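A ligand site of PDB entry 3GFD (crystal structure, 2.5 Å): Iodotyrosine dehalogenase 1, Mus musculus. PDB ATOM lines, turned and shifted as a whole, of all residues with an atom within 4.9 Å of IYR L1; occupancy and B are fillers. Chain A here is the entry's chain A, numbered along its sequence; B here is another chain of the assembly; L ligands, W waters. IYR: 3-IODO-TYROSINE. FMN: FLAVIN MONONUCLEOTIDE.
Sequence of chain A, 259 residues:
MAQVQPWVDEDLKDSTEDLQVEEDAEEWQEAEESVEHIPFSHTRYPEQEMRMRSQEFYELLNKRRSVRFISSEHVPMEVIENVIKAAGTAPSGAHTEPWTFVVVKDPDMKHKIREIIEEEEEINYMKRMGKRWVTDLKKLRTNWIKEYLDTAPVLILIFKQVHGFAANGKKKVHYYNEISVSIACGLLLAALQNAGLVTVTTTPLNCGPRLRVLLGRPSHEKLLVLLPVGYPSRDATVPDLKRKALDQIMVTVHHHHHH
The side-chain hydroxyl of Tyr 125 lies within hydrogen-bond range of an oxygen (OXT) of IYR L1. The backbone NH (N) of Ala 94 of chain B sits at hydrogen-bond distance from an oxygen (OF) of IYR L1 (2.8 Å). The side-chain amino group (NZ) of Lys 146 lies within salt-bridge range of an oxygen (OXT) of IYR L1, 2.8 Å away. N of IYR L1 is in salt-bridge range of OE2 of Glu 121, 2.8 Å away. O of Thr 203 is in hydrogen-bond range of N of IYR L1 (3.4 Å). An oxygen (O4) of FMN L2 sits at hydrogen-bond distance from the backbone NH (N) of Thr 203. The side-chain hydroxyl of Thr 203 lies within hydrogen-bond range of a nitrogen (N5) of FMN L2 (3.1 Å). O2 of FMN L2 sits at hydrogen-bond distance from NE of Arg 68. The backbone NH (N) of Ser 92 of chain B sits at hydrogen-bond distance from an oxygen (O3') of FMN L2 (3.3 Å).
An oxygen (OF) of IYR L1 sits at hydrogen-bond distance from an oxygen (O2') of FMN L2 (2.5 Å).
The side-chain hydroxyl (OH) of Tyr 125 lies within hydrogen-bond range of the side-chain hydroxyl (OG1) of Thr 142. The backbone carbonyl oxygen (O) of Asn 143 sits at hydrogen-bond distance from the side-chain amino group (NZ) of Lys 146, 2.9 Å away. N of Trp 133 lies close to OH of Tyr 175 of chain B, at 3.4 Å.
The backbone carbonyl oxygen of Asn 143 lies close to an oxygen (OXT) of IYR L1, at 3.5 Å. Trp 133 touches IYR L1. CD2 of Leu 137 touches CF of IYR L1, at 3.5 Å. CD2 of Leu 140 touches OF of IYR L1, 3.998 Å away. Thr 142 touches IYR L1. Gly 93 of chain B touches IYR L1 (CA to IE, 3.7 Å). Tyr 175 of chain B touches IYR L1. CD1 of Tyr 176 of chain B touches IE of IYR L1, at 3.8 Å. 13 residues have an atom within 4 Å of IYR L1: Glu 121, Tyr 125, Trp 133, Leu 137, Leu 140, Thr 142, Asn 143, Lys 146, Thr 203, Gly 93 of chain B, Ala 94 of chain B, Tyr 175 of chain B and Tyr 176 of chain B. The nearest printed residue that does not touch IYR L1 is Met 129 (4.03 Å).
Water W3 bridges O of IYR L1 and OE2 of Glu 121. Water W1 lies within hydrogen-bond range of the side-chain carboxylate (OE1) of Glu 121, a nitrogen (N) of IYR L1 and the side-chain sulfur (SD) of Met 129. Water W2 lies within hydrogen-bond range of O of Thr 203, OH of Tyr 176 of chain B and N of IYR L1.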
ATOM      1  N   ARG A  68      -7.257 -15.049   6.406  1.00  0.00           N
ATOM      2  CA  ARG A  68      -6.519 -15.605   5.295  1.00  0.00           C
ATOM      3  C   ARG A  68      -5.724 -14.577   4.456  1.00  0.00           C
ATOM      4  O   ARG A  68      -5.201 -14.895   3.368  1.00  0.00           O
ATOM      5  CB  ARG A  68      -7.479 -16.399   4.435  1.00  0.00           C
ATOM      6  CG  ARG A  68      -8.095 -17.572   5.171  1.00  0.00           C
ATOM      7  CD  ARG A  68      -9.094 -18.336   4.327  1.00  0.00           C
ATOM      8  NE  ARG A  68      -9.494 -19.551   5.058  1.00  0.00           N
ATOM      9  CZ  ARG A  68     -10.620 -19.651   5.764  1.00  0.00           C
ATOM     10  NH1 ARG A  68     -11.489 -18.625   5.822  1.00  0.00           N
ATOM     11  NH2 ARG A  68     -10.907 -20.766   6.404  1.00  0.00           N
ATOM     12  N   GLU A 121      -2.752 -28.426  -3.460  1.00  0.00           N
ATOM     13  CA  GLU A 121      -4.143 -27.998  -3.226  1.00  0.00           C
ATOM     14  C   GLU A 121      -4.927 -27.944  -4.522  1.00  0.00           C
ATOM     15  O   GLU A 121      -6.133 -28.175  -4.538  1.00  0.00           O
ATOM     16  CB  GLU A 121      -4.243 -26.636  -2.522  1.00  0.00           C
ATOM     17  CG  GLU A 121      -3.898 -26.582  -1.018  1.00  0.00           C
ATOM     18  CD  GLU A 121      -4.792 -27.445  -0.121  1.00  0.00           C
ATOM     19  OE1 GLU A 121      -5.557 -28.308  -0.642  1.00  0.00           O
ATOM     20  OE2 GLU A 121      -4.722 -27.254   1.126  1.00  0.00           O
ATOM     21  N   TYR A 125      -8.510 -29.473  -4.985  1.00  0.00           N
ATOM     22  CA  TYR A 125      -9.714 -28.786  -5.442  1.00  0.00           C
ATOM     23  C   TYR A 125     -10.304 -29.379  -6.727  1.00  0.00           C
ATOM     24  O   TYR A 125     -11.521 -29.538  -6.856  1.00  0.00           O
ATOM     25  CB  TYR A 125      -9.466 -27.289  -5.633  1.00  0.00           C
ATOM     26  CG  TYR A 125      -9.668 -26.484  -4.377  1.00  0.00           C
ATOM     27  CD1 TYR A 125      -8.596 -26.267  -3.503  1.00  0.00           C
ATOM     28  CD2 TYR A 125     -10.922 -25.952  -4.047  1.00  0.00           C
ATOM     29  CE1 TYR A 125      -8.752 -25.530  -2.345  1.00  0.00           C
ATOM     30  CE2 TYR A 125     -11.087 -25.200  -2.874  1.00  0.00           C
ATOM     31  CZ  TYR A 125      -9.999 -25.003  -2.010  1.00  0.00           C
ATOM     32  OH  TYR A 125     -10.098 -24.275  -0.842  1.00  0.00           O
ATOM     33  N   MET A 129     -10.412 -33.797  -3.037  1.00  0.00           N
ATOM     34  CA  MET A 129     -11.407 -33.624  -1.993  1.00  0.00           C
ATOM     35  C   MET A 129     -12.795 -34.217  -2.367  1.00  0.00           C
ATOM     36  O   MET A 129     -13.481 -34.738  -1.488  1.00  0.00           O
ATOM     37  CB  MET A 129     -11.503 -32.149  -1.563  1.00  0.00           C
ATOM     38  CG  MET A 129     -10.274 -31.672  -0.828  1.00  0.00           C
ATOM     39  SD  MET A 129     -10.339 -29.973  -0.223  1.00  0.00           S
ATOM     40  CE  MET A 129     -10.229 -29.002  -1.721  1.00  0.00           C
ATOM     41  N   TRP A 133     -17.085 -32.034  -0.567  1.00  0.00           N
ATOM     42  CA  TRP A 133     -16.160 -31.221   0.169  1.00  0.00           C
ATOM     43  C   TRP A 133     -15.967 -29.869  -0.557  1.00  0.00           C
ATOM     44  O   TRP A 133     -16.108 -28.798   0.047  1.00  0.00           O
ATOM     45  CB  TRP A 133     -14.854 -31.985   0.340  1.00  0.00           C
ATOM     46  CG  TRP A 133     -13.868 -31.414   1.340  1.00  0.00           C
ATOM     47  CD1 TRP A 133     -13.897 -30.181   1.934  1.00  0.00           C
ATOM     48  CD2 TRP A 133     -12.668 -32.071   1.827  1.00  0.00           C
ATOM     49  NE1 TRP A 133     -12.806 -30.039   2.812  1.00  0.00           N
ATOM     50  CE2 TRP A 133     -12.037 -31.163   2.735  1.00  0.00           C
ATOM     51  CE3 TRP A 133     -12.094 -33.331   1.607  1.00  0.00           C
ATOM     52  CZ2 TRP A 133     -10.846 -31.472   3.380  1.00  0.00           C
ATOM     53  CZ3 TRP A 133     -10.911 -33.635   2.248  1.00  0.00           C
ATOM     54  CH2 TRP A 133     -10.295 -32.701   3.144  1.00  0.00           C
ATOM     55  N   LEU A 137     -16.876 -25.947   0.900  1.00  0.00           N
ATOM     56  CA  LEU A 137     -15.945 -24.836   1.043  1.00  0.00           C
ATOM     57  C   LEU A 137     -16.384 -23.537   0.360  1.00  0.00           C
ATOM     58  O   LEU A 137     -15.777 -22.468   0.614  1.00  0.00           O
ATOM     59  CB  LEU A 137     -14.555 -25.247   0.580  1.00  0.00           C
ATOM     60  CG  LEU A 137     -13.988 -26.440   1.380  1.00  0.00           C
ATOM     61  CD1 LEU A 137     -12.758 -26.981   0.652  1.00  0.00           C
ATOM     62  CD2 LEU A 137     -13.686 -26.094   2.843  1.00  0.00           C
ATOM     63  N   LEU A 140     -16.652 -20.260   2.168  1.00  0.00           N
ATOM     64  CA  LEU A 140     -15.413 -19.744   2.719  1.00  0.00           C
ATOM     65  C   LEU A 140     -14.625 -19.024   1.624  1.00  0.00           C
ATOM     66  O   LEU A 140     -13.704 -18.257   1.917  1.00  0.00           O
ATOM     67  CB  LEU A 140     -14.631 -20.928   3.259  1.00  0.00           C
ATOM     68  CG  LEU A 140     -14.792 -21.366   4.713  1.00  0.00           C
ATOM     69  CD1 LEU A 140     -16.028 -20.913   5.503  1.00  0.00           C
ATOM     70  CD2 LEU A 140     -14.594 -22.856   4.908  1.00  0.00           C
ATOM     71  N   THR A 142     -12.364 -20.198  -0.262  1.00  0.00           N
ATOM     72  CA  THR A 142     -10.952 -20.576  -0.340  1.00  0.00           C
ATOM     73  C   THR A 142     -10.646 -21.206  -1.712  1.00  0.00           C
ATOM     74  O   THR A 142     -11.514 -21.787  -2.341  1.00  0.00           O
ATOM     75  CB  THR A 142     -10.644 -21.575   0.756  1.00  0.00           C
ATOM     76  OG1 THR A 142     -11.675 -22.569   0.737  1.00  0.00           O
ATOM     77  CG2 THR A 142     -10.661 -20.887   2.117  1.00  0.00           C
ATOM     78  N   ASN A 143      -9.409 -21.108  -2.162  1.00  0.00           N
ATOM     79  CA  ASN A 143      -9.017 -21.820  -3.366  1.00  0.00           C
ATOM     80  C   ASN A 143      -7.599 -22.289  -3.123  1.00  0.00           C
ATOM     81  O   ASN A 143      -7.142 -22.296  -1.957  1.00  0.00           O
ATOM     82  CB  ASN A 143      -9.144 -20.932  -4.625  1.00  0.00           C
ATOM     83  CG  ASN A 143      -8.342 -19.646  -4.520  1.00  0.00           C
ATOM     84  OD1 ASN A 143      -7.280 -19.568  -3.892  1.00  0.00           O
ATOM     85  ND2 ASN A 143      -8.877 -18.611  -5.111  1.00  0.00           N
ATOM     86  N   LYS A 146      -2.371 -19.470  -2.202  1.00  0.00           N
ATOM     87  CA  LYS A 146      -2.109 -19.200  -0.818  1.00  0.00           C
ATOM     88  C   LYS A 146      -1.000 -18.185  -0.691  1.00  0.00           C
ATOM     89  O   LYS A 146       0.138 -18.474  -0.249  1.00  0.00           O
ATOM     90  CB  LYS A 146      -1.741 -20.480  -0.040  1.00  0.00           C
ATOM     91  CG  LYS A 146      -2.761 -21.576  -0.143  1.00  0.00           C
ATOM     92  CD  LYS A 146      -4.083 -21.162   0.470  1.00  0.00           C
ATOM     93  CE  LYS A 146      -5.074 -22.346   0.444  1.00  0.00           C
ATOM     94  NZ  LYS A 146      -6.475 -21.931   0.849  1.00  0.00           N
ATOM     95  N   TYR A 148      -0.607 -15.933   1.405  1.00  0.00           N
ATOM     96  CA  TYR A 148      -0.103 -15.771   2.762  1.00  0.00           C
ATOM     97  C   TYR A 148       1.173 -16.614   3.033  1.00  0.00           C
ATOM     98  O   TYR A 148       1.961 -16.241   3.875  1.00  0.00           O
ATOM     99  CB  TYR A 148      -1.180 -16.041   3.851  1.00  0.00           C
ATOM    100  CG  TYR A 148      -1.832 -17.413   3.801  1.00  0.00           C
ATOM    101  CD1 TYR A 148      -3.175 -17.555   3.420  1.00  0.00           C
ATOM    102  CD2 TYR A 148      -1.117 -18.570   4.156  1.00  0.00           C
ATOM    103  CE1 TYR A 148      -3.806 -18.836   3.396  1.00  0.00           C
ATOM    104  CE2 TYR A 148      -1.714 -19.834   4.149  1.00  0.00           C
ATOM    105  CZ  TYR A 148      -3.053 -19.961   3.783  1.00  0.00           C
ATOM    106  OH  TYR A 148      -3.613 -21.229   3.749  1.00  0.00           O
ATOM    107  N   THR A 203      -4.837 -27.298   7.043  1.00  0.00           N
ATOM    108  CA  THR A 203      -4.478 -28.705   6.872  1.00  0.00           C
ATOM    109  C   THR A 203      -4.231 -28.908   5.350  1.00  0.00           C
ATOM    110  O   THR A 203      -5.141 -29.220   4.579  1.00  0.00           O
ATOM    111  CB  THR A 203      -5.634 -29.623   7.271  1.00  0.00           C
ATOM    112  OG1 THR A 203      -6.849 -29.099   6.701  1.00  0.00           O
ATOM    113  CG2 THR A 203      -5.748 -29.708   8.774  1.00  0.00           C
ATOM    114  N   PRO A 204      -2.983 -28.766   4.924  1.00  0.00           N
ATOM    115  CA  PRO A 204      -2.704 -28.915   3.512  1.00  0.00           C
ATOM    116  C   PRO A 204      -2.673 -30.421   3.135  1.00  0.00           C
ATOM    117  O   PRO A 204      -1.617 -31.092   3.238  1.00  0.00           O
ATOM    118  CB  PRO A 204      -1.328 -28.272   3.363  1.00  0.00           C
ATOM    119  CG  PRO A 204      -0.826 -28.009   4.783  1.00  0.00           C
ATOM    120  CD  PRO A 204      -1.795 -28.537   5.749  1.00  0.00           C
ATOM    121  N   SER B  92     -13.015 -24.809  13.288  1.00  0.00           N
ATOM    122  CA  SER B  92     -13.352 -26.171  12.974  1.00  0.00           C
ATOM    123  C   SER B  92     -13.356 -26.374  11.484  1.00  0.00           C
ATOM    124  O   SER B  92     -13.679 -25.439  10.683  1.00  0.00           O
ATOM    125  CB  SER B  92     -14.715 -26.574  13.567  1.00  0.00           C
ATOM    126  OG  SER B  92     -15.792 -25.839  12.955  1.00  0.00           O
ATOM    127  N   GLY B  93     -13.042 -27.590  11.075  1.00  0.00           N
ATOM    128  CA  GLY B  93     -12.937 -27.869   9.630  1.00  0.00           C
ATOM    129  C   GLY B  93     -14.233 -27.508   8.918  1.00  0.00           C
ATOM    130  O   GLY B  93     -15.309 -27.983   9.306  1.00  0.00           O
ATOM    131  N   ALA B  94     -14.130 -26.670   7.870  1.00  0.00           N
ATOM    132  CA  ALA B  94     -15.317 -26.187   7.111  1.00  0.00           C
ATOM    133  C   ALA B  94     -16.453 -25.608   7.996  1.00  0.00           C
ATOM    134  O   ALA B  94     -17.624 -25.694   7.638  1.00  0.00           O
ATOM    135  CB  ALA B  94     -15.869 -27.281   6.153  1.00  0.00           C
ATOM    136  N   HIS B  95     -16.104 -24.990   9.136  1.00  0.00           N
ATOM    137  CA  HIS B  95     -17.101 -24.407  10.054  1.00  0.00           C
ATOM    138  C   HIS B  95     -18.210 -25.381  10.429  1.00  0.00           C
ATOM    139  O   HIS B  95     -19.401 -25.101  10.253  1.00  0.00           O
ATOM    140  CB  HIS B  95     -17.690 -23.091   9.482  1.00  0.00           C
ATOM    141  CG  HIS B  95     -18.600 -22.348  10.434  1.00  0.00           C
ATOM    142  ND1 HIS B  95     -18.229 -22.032  11.729  1.00  0.00           N
ATOM    143  CD2 HIS B  95     -19.867 -21.883  10.274  1.00  0.00           C
ATOM    144  CE1 HIS B  95     -19.236 -21.411  12.329  1.00  0.00           C
ATOM    145  NE2 HIS B  95     -20.229 -21.295  11.461  1.00  0.00           N
ATOM    146  N   TYR B 175     -15.323 -32.583   8.689  1.00  0.00           N
ATOM    147  CA  TYR B 175     -13.923 -32.650   8.309  1.00  0.00           C
ATOM    148  C   TYR B 175     -13.043 -32.435   9.522  1.00  0.00           C
ATOM    149  O   TYR B 175     -13.216 -31.456  10.266  1.00  0.00           O
ATOM    150  CB  TYR B 175     -13.607 -31.626   7.194  1.00  0.00           C
ATOM    151  CG  TYR B 175     -14.587 -31.759   6.011  1.00  0.00           C
ATOM    152  CD1 TYR B 175     -14.363 -32.682   4.969  1.00  0.00           C
ATOM    153  CD2 TYR B 175     -15.759 -30.982   5.958  1.00  0.00           C
ATOM    154  CE1 TYR B 175     -15.279 -32.815   3.914  1.00  0.00           C
ATOM    155  CE2 TYR B 175     -16.697 -31.111   4.899  1.00  0.00           C
ATOM    156  CZ  TYR B 175     -16.447 -32.023   3.877  1.00  0.00           C
ATOM    157  OH  TYR B 175     -17.374 -32.147   2.861  1.00  0.00           O
ATOM    158  N   TYR B 176     -12.099 -33.341   9.713  1.00  0.00           N
ATOM    159  CA  TYR B 176     -11.138 -33.248  10.780  1.00  0.00           C
ATOM    160  C   TYR B 176     -11.851 -33.025  12.127  1.00  0.00           C
ATOM    161  O   TYR B 176     -11.415 -32.182  12.925  1.00  0.00           O
ATOM    162  CB  TYR B 176     -10.117 -32.141  10.524  1.00  0.00           C
ATOM    163  CG  TYR B 176      -9.413 -32.245   9.197  1.00  0.00           C
ATOM    164  CD1 TYR B 176      -9.717 -31.378   8.153  1.00  0.00           C
ATOM    165  CD2 TYR B 176      -8.407 -33.167   9.004  1.00  0.00           C
ATOM    166  CE1 TYR B 176      -9.056 -31.461   6.924  1.00  0.00           C
ATOM    167  CE2 TYR B 176      -7.710 -33.271   7.777  1.00  0.00           C
ATOM    168  CZ  TYR B 176      -8.041 -32.418   6.736  1.00  0.00           C
ATOM    169  OH  TYR B 176      -7.360 -32.515   5.527  1.00  0.00           O
HETATM  170  N   IYR L   1      -7.060 -27.187   2.626  1.00  0.00           N
HETATM  171  CA  IYR L   1      -7.754 -26.421   1.558  1.00  0.00           C
HETATM  172  CB  IYR L   1      -9.243 -26.592   1.687  1.00  0.00           C
HETATM  173  CC  IYR L   1      -9.927 -26.220   3.000  1.00  0.00           C
HETATM  174  CD  IYR L   1     -10.316 -27.268   3.854  1.00  0.00           C
HETATM  175  CE  IYR L   1     -10.993 -27.026   5.073  1.00  0.00           C
HETATM  176  IE  IYR L   1     -11.601 -28.626   6.298  1.00  0.00           I
HETATM  177  CF  IYR L   1     -11.348 -25.644   5.423  1.00  0.00           C
HETATM  178  OF  IYR L   1     -12.021 -25.411   6.591  1.00  0.00           O
HETATM  179  CG  IYR L   1     -10.962 -24.607   4.530  1.00  0.00           C
HETATM  180  CH  IYR L   1     -10.243 -24.881   3.340  1.00  0.00           C
HETATM  181  C   IYR L   1      -7.477 -24.930   1.584  1.00  0.00           C
HETATM  182  O   IYR L   1      -6.643 -24.424   2.356  1.00  0.00           O
HETATM  183  OXT IYR L   1      -8.112 -24.170   0.814  1.00  0.00           O
HETATM  184  N1  FMN L   2      -8.942 -22.898   6.568  1.00  0.00           N
HETATM  185  C2  FMN L   2      -8.331 -22.894   5.360  1.00  0.00           C
HETATM  186  O2  FMN L   2      -8.340 -21.831   4.728  1.00  0.00           O
HETATM  187  N3  FMN L   2      -7.750 -23.995   4.878  1.00  0.00           N
HETATM  188  C4  FMN L   2      -7.718 -25.210   5.517  1.00  0.00           C
HETATM  189  O4  FMN L   2      -7.077 -26.276   5.289  1.00  0.00           O
HETATM  190  C4A FMN L   2      -8.318 -25.201   6.753  1.00  0.00           C
HETATM  191  N5  FMN L   2      -8.276 -26.443   7.383  1.00  0.00           N
HETATM  192  C5A FMN L   2      -8.766 -26.518   8.647  1.00  0.00           C
HETATM  193  C6  FMN L   2      -8.669 -27.695   9.330  1.00  0.00           C
HETATM  194  C7  FMN L   2      -9.168 -27.820  10.671  1.00  0.00           C
HETATM  195  C7M FMN L   2      -8.712 -28.898  11.641  1.00  0.00           C
HETATM  196  C8  FMN L   2      -9.767 -26.692  11.294  1.00  0.00           C
HETATM  197  C8M FMN L   2      -9.760 -26.688  12.812  1.00  0.00           C
HETATM  198  C9  FMN L   2      -9.835 -25.479  10.553  1.00  0.00           C
HETATM  199  C9A FMN L   2      -9.364 -25.386   9.246  1.00  0.00           C
HETATM  200  N10 FMN L   2      -9.445 -24.150   8.571  1.00  0.00           N
HETATM  201  C10 FMN L   2      -8.905 -24.070   7.298  1.00  0.00           C
HETATM  202  C1' FMN L   2     -10.244 -23.002   9.298  1.00  0.00           C
HETATM  203  C2' FMN L   2     -11.759 -23.222   9.226  1.00  0.00           C
HETATM  204  O2' FMN L   2     -12.161 -23.220   7.879  1.00  0.00           O
HETATM  205  C3' FMN L   2     -12.403 -22.129  10.027  1.00  0.00           C
HETATM  206  O3' FMN L   2     -12.068 -22.325  11.381  1.00  0.00           O
HETATM  207  C4' FMN L   2     -13.927 -22.104   9.961  1.00  0.00           C
HETATM  208  O4' FMN L   2     -14.291 -21.725   8.663  1.00  0.00           O
HETATM  209  C5' FMN L   2     -14.591 -21.233  11.053  1.00  0.00           C
HETATM  210  O5' FMN L   2     -13.970 -19.965  11.016  1.00  0.00           O
HETATM  211  P   FMN L   2     -13.344 -19.251  12.292  1.00  0.00           P
HETATM  212  O1P FMN L   2     -13.120 -17.787  11.949  1.00  0.00           O
HETATM  213  O2P FMN L   2     -11.998 -19.910  12.617  1.00  0.00           O
HETATM  214  O3P FMN L   2     -14.255 -19.352  13.495  1.00  0.00           O
HETATM  215  O   HOH W   1      -7.363 -29.736   1.154  1.00  0.00           O
HETATM  216  O   HOH W   2      -7.702 -30.250   3.768  1.00  0.00           O
HETATM  217  O   HOH W   3      -4.007 -25.022   2.663  1.00  0.00           O
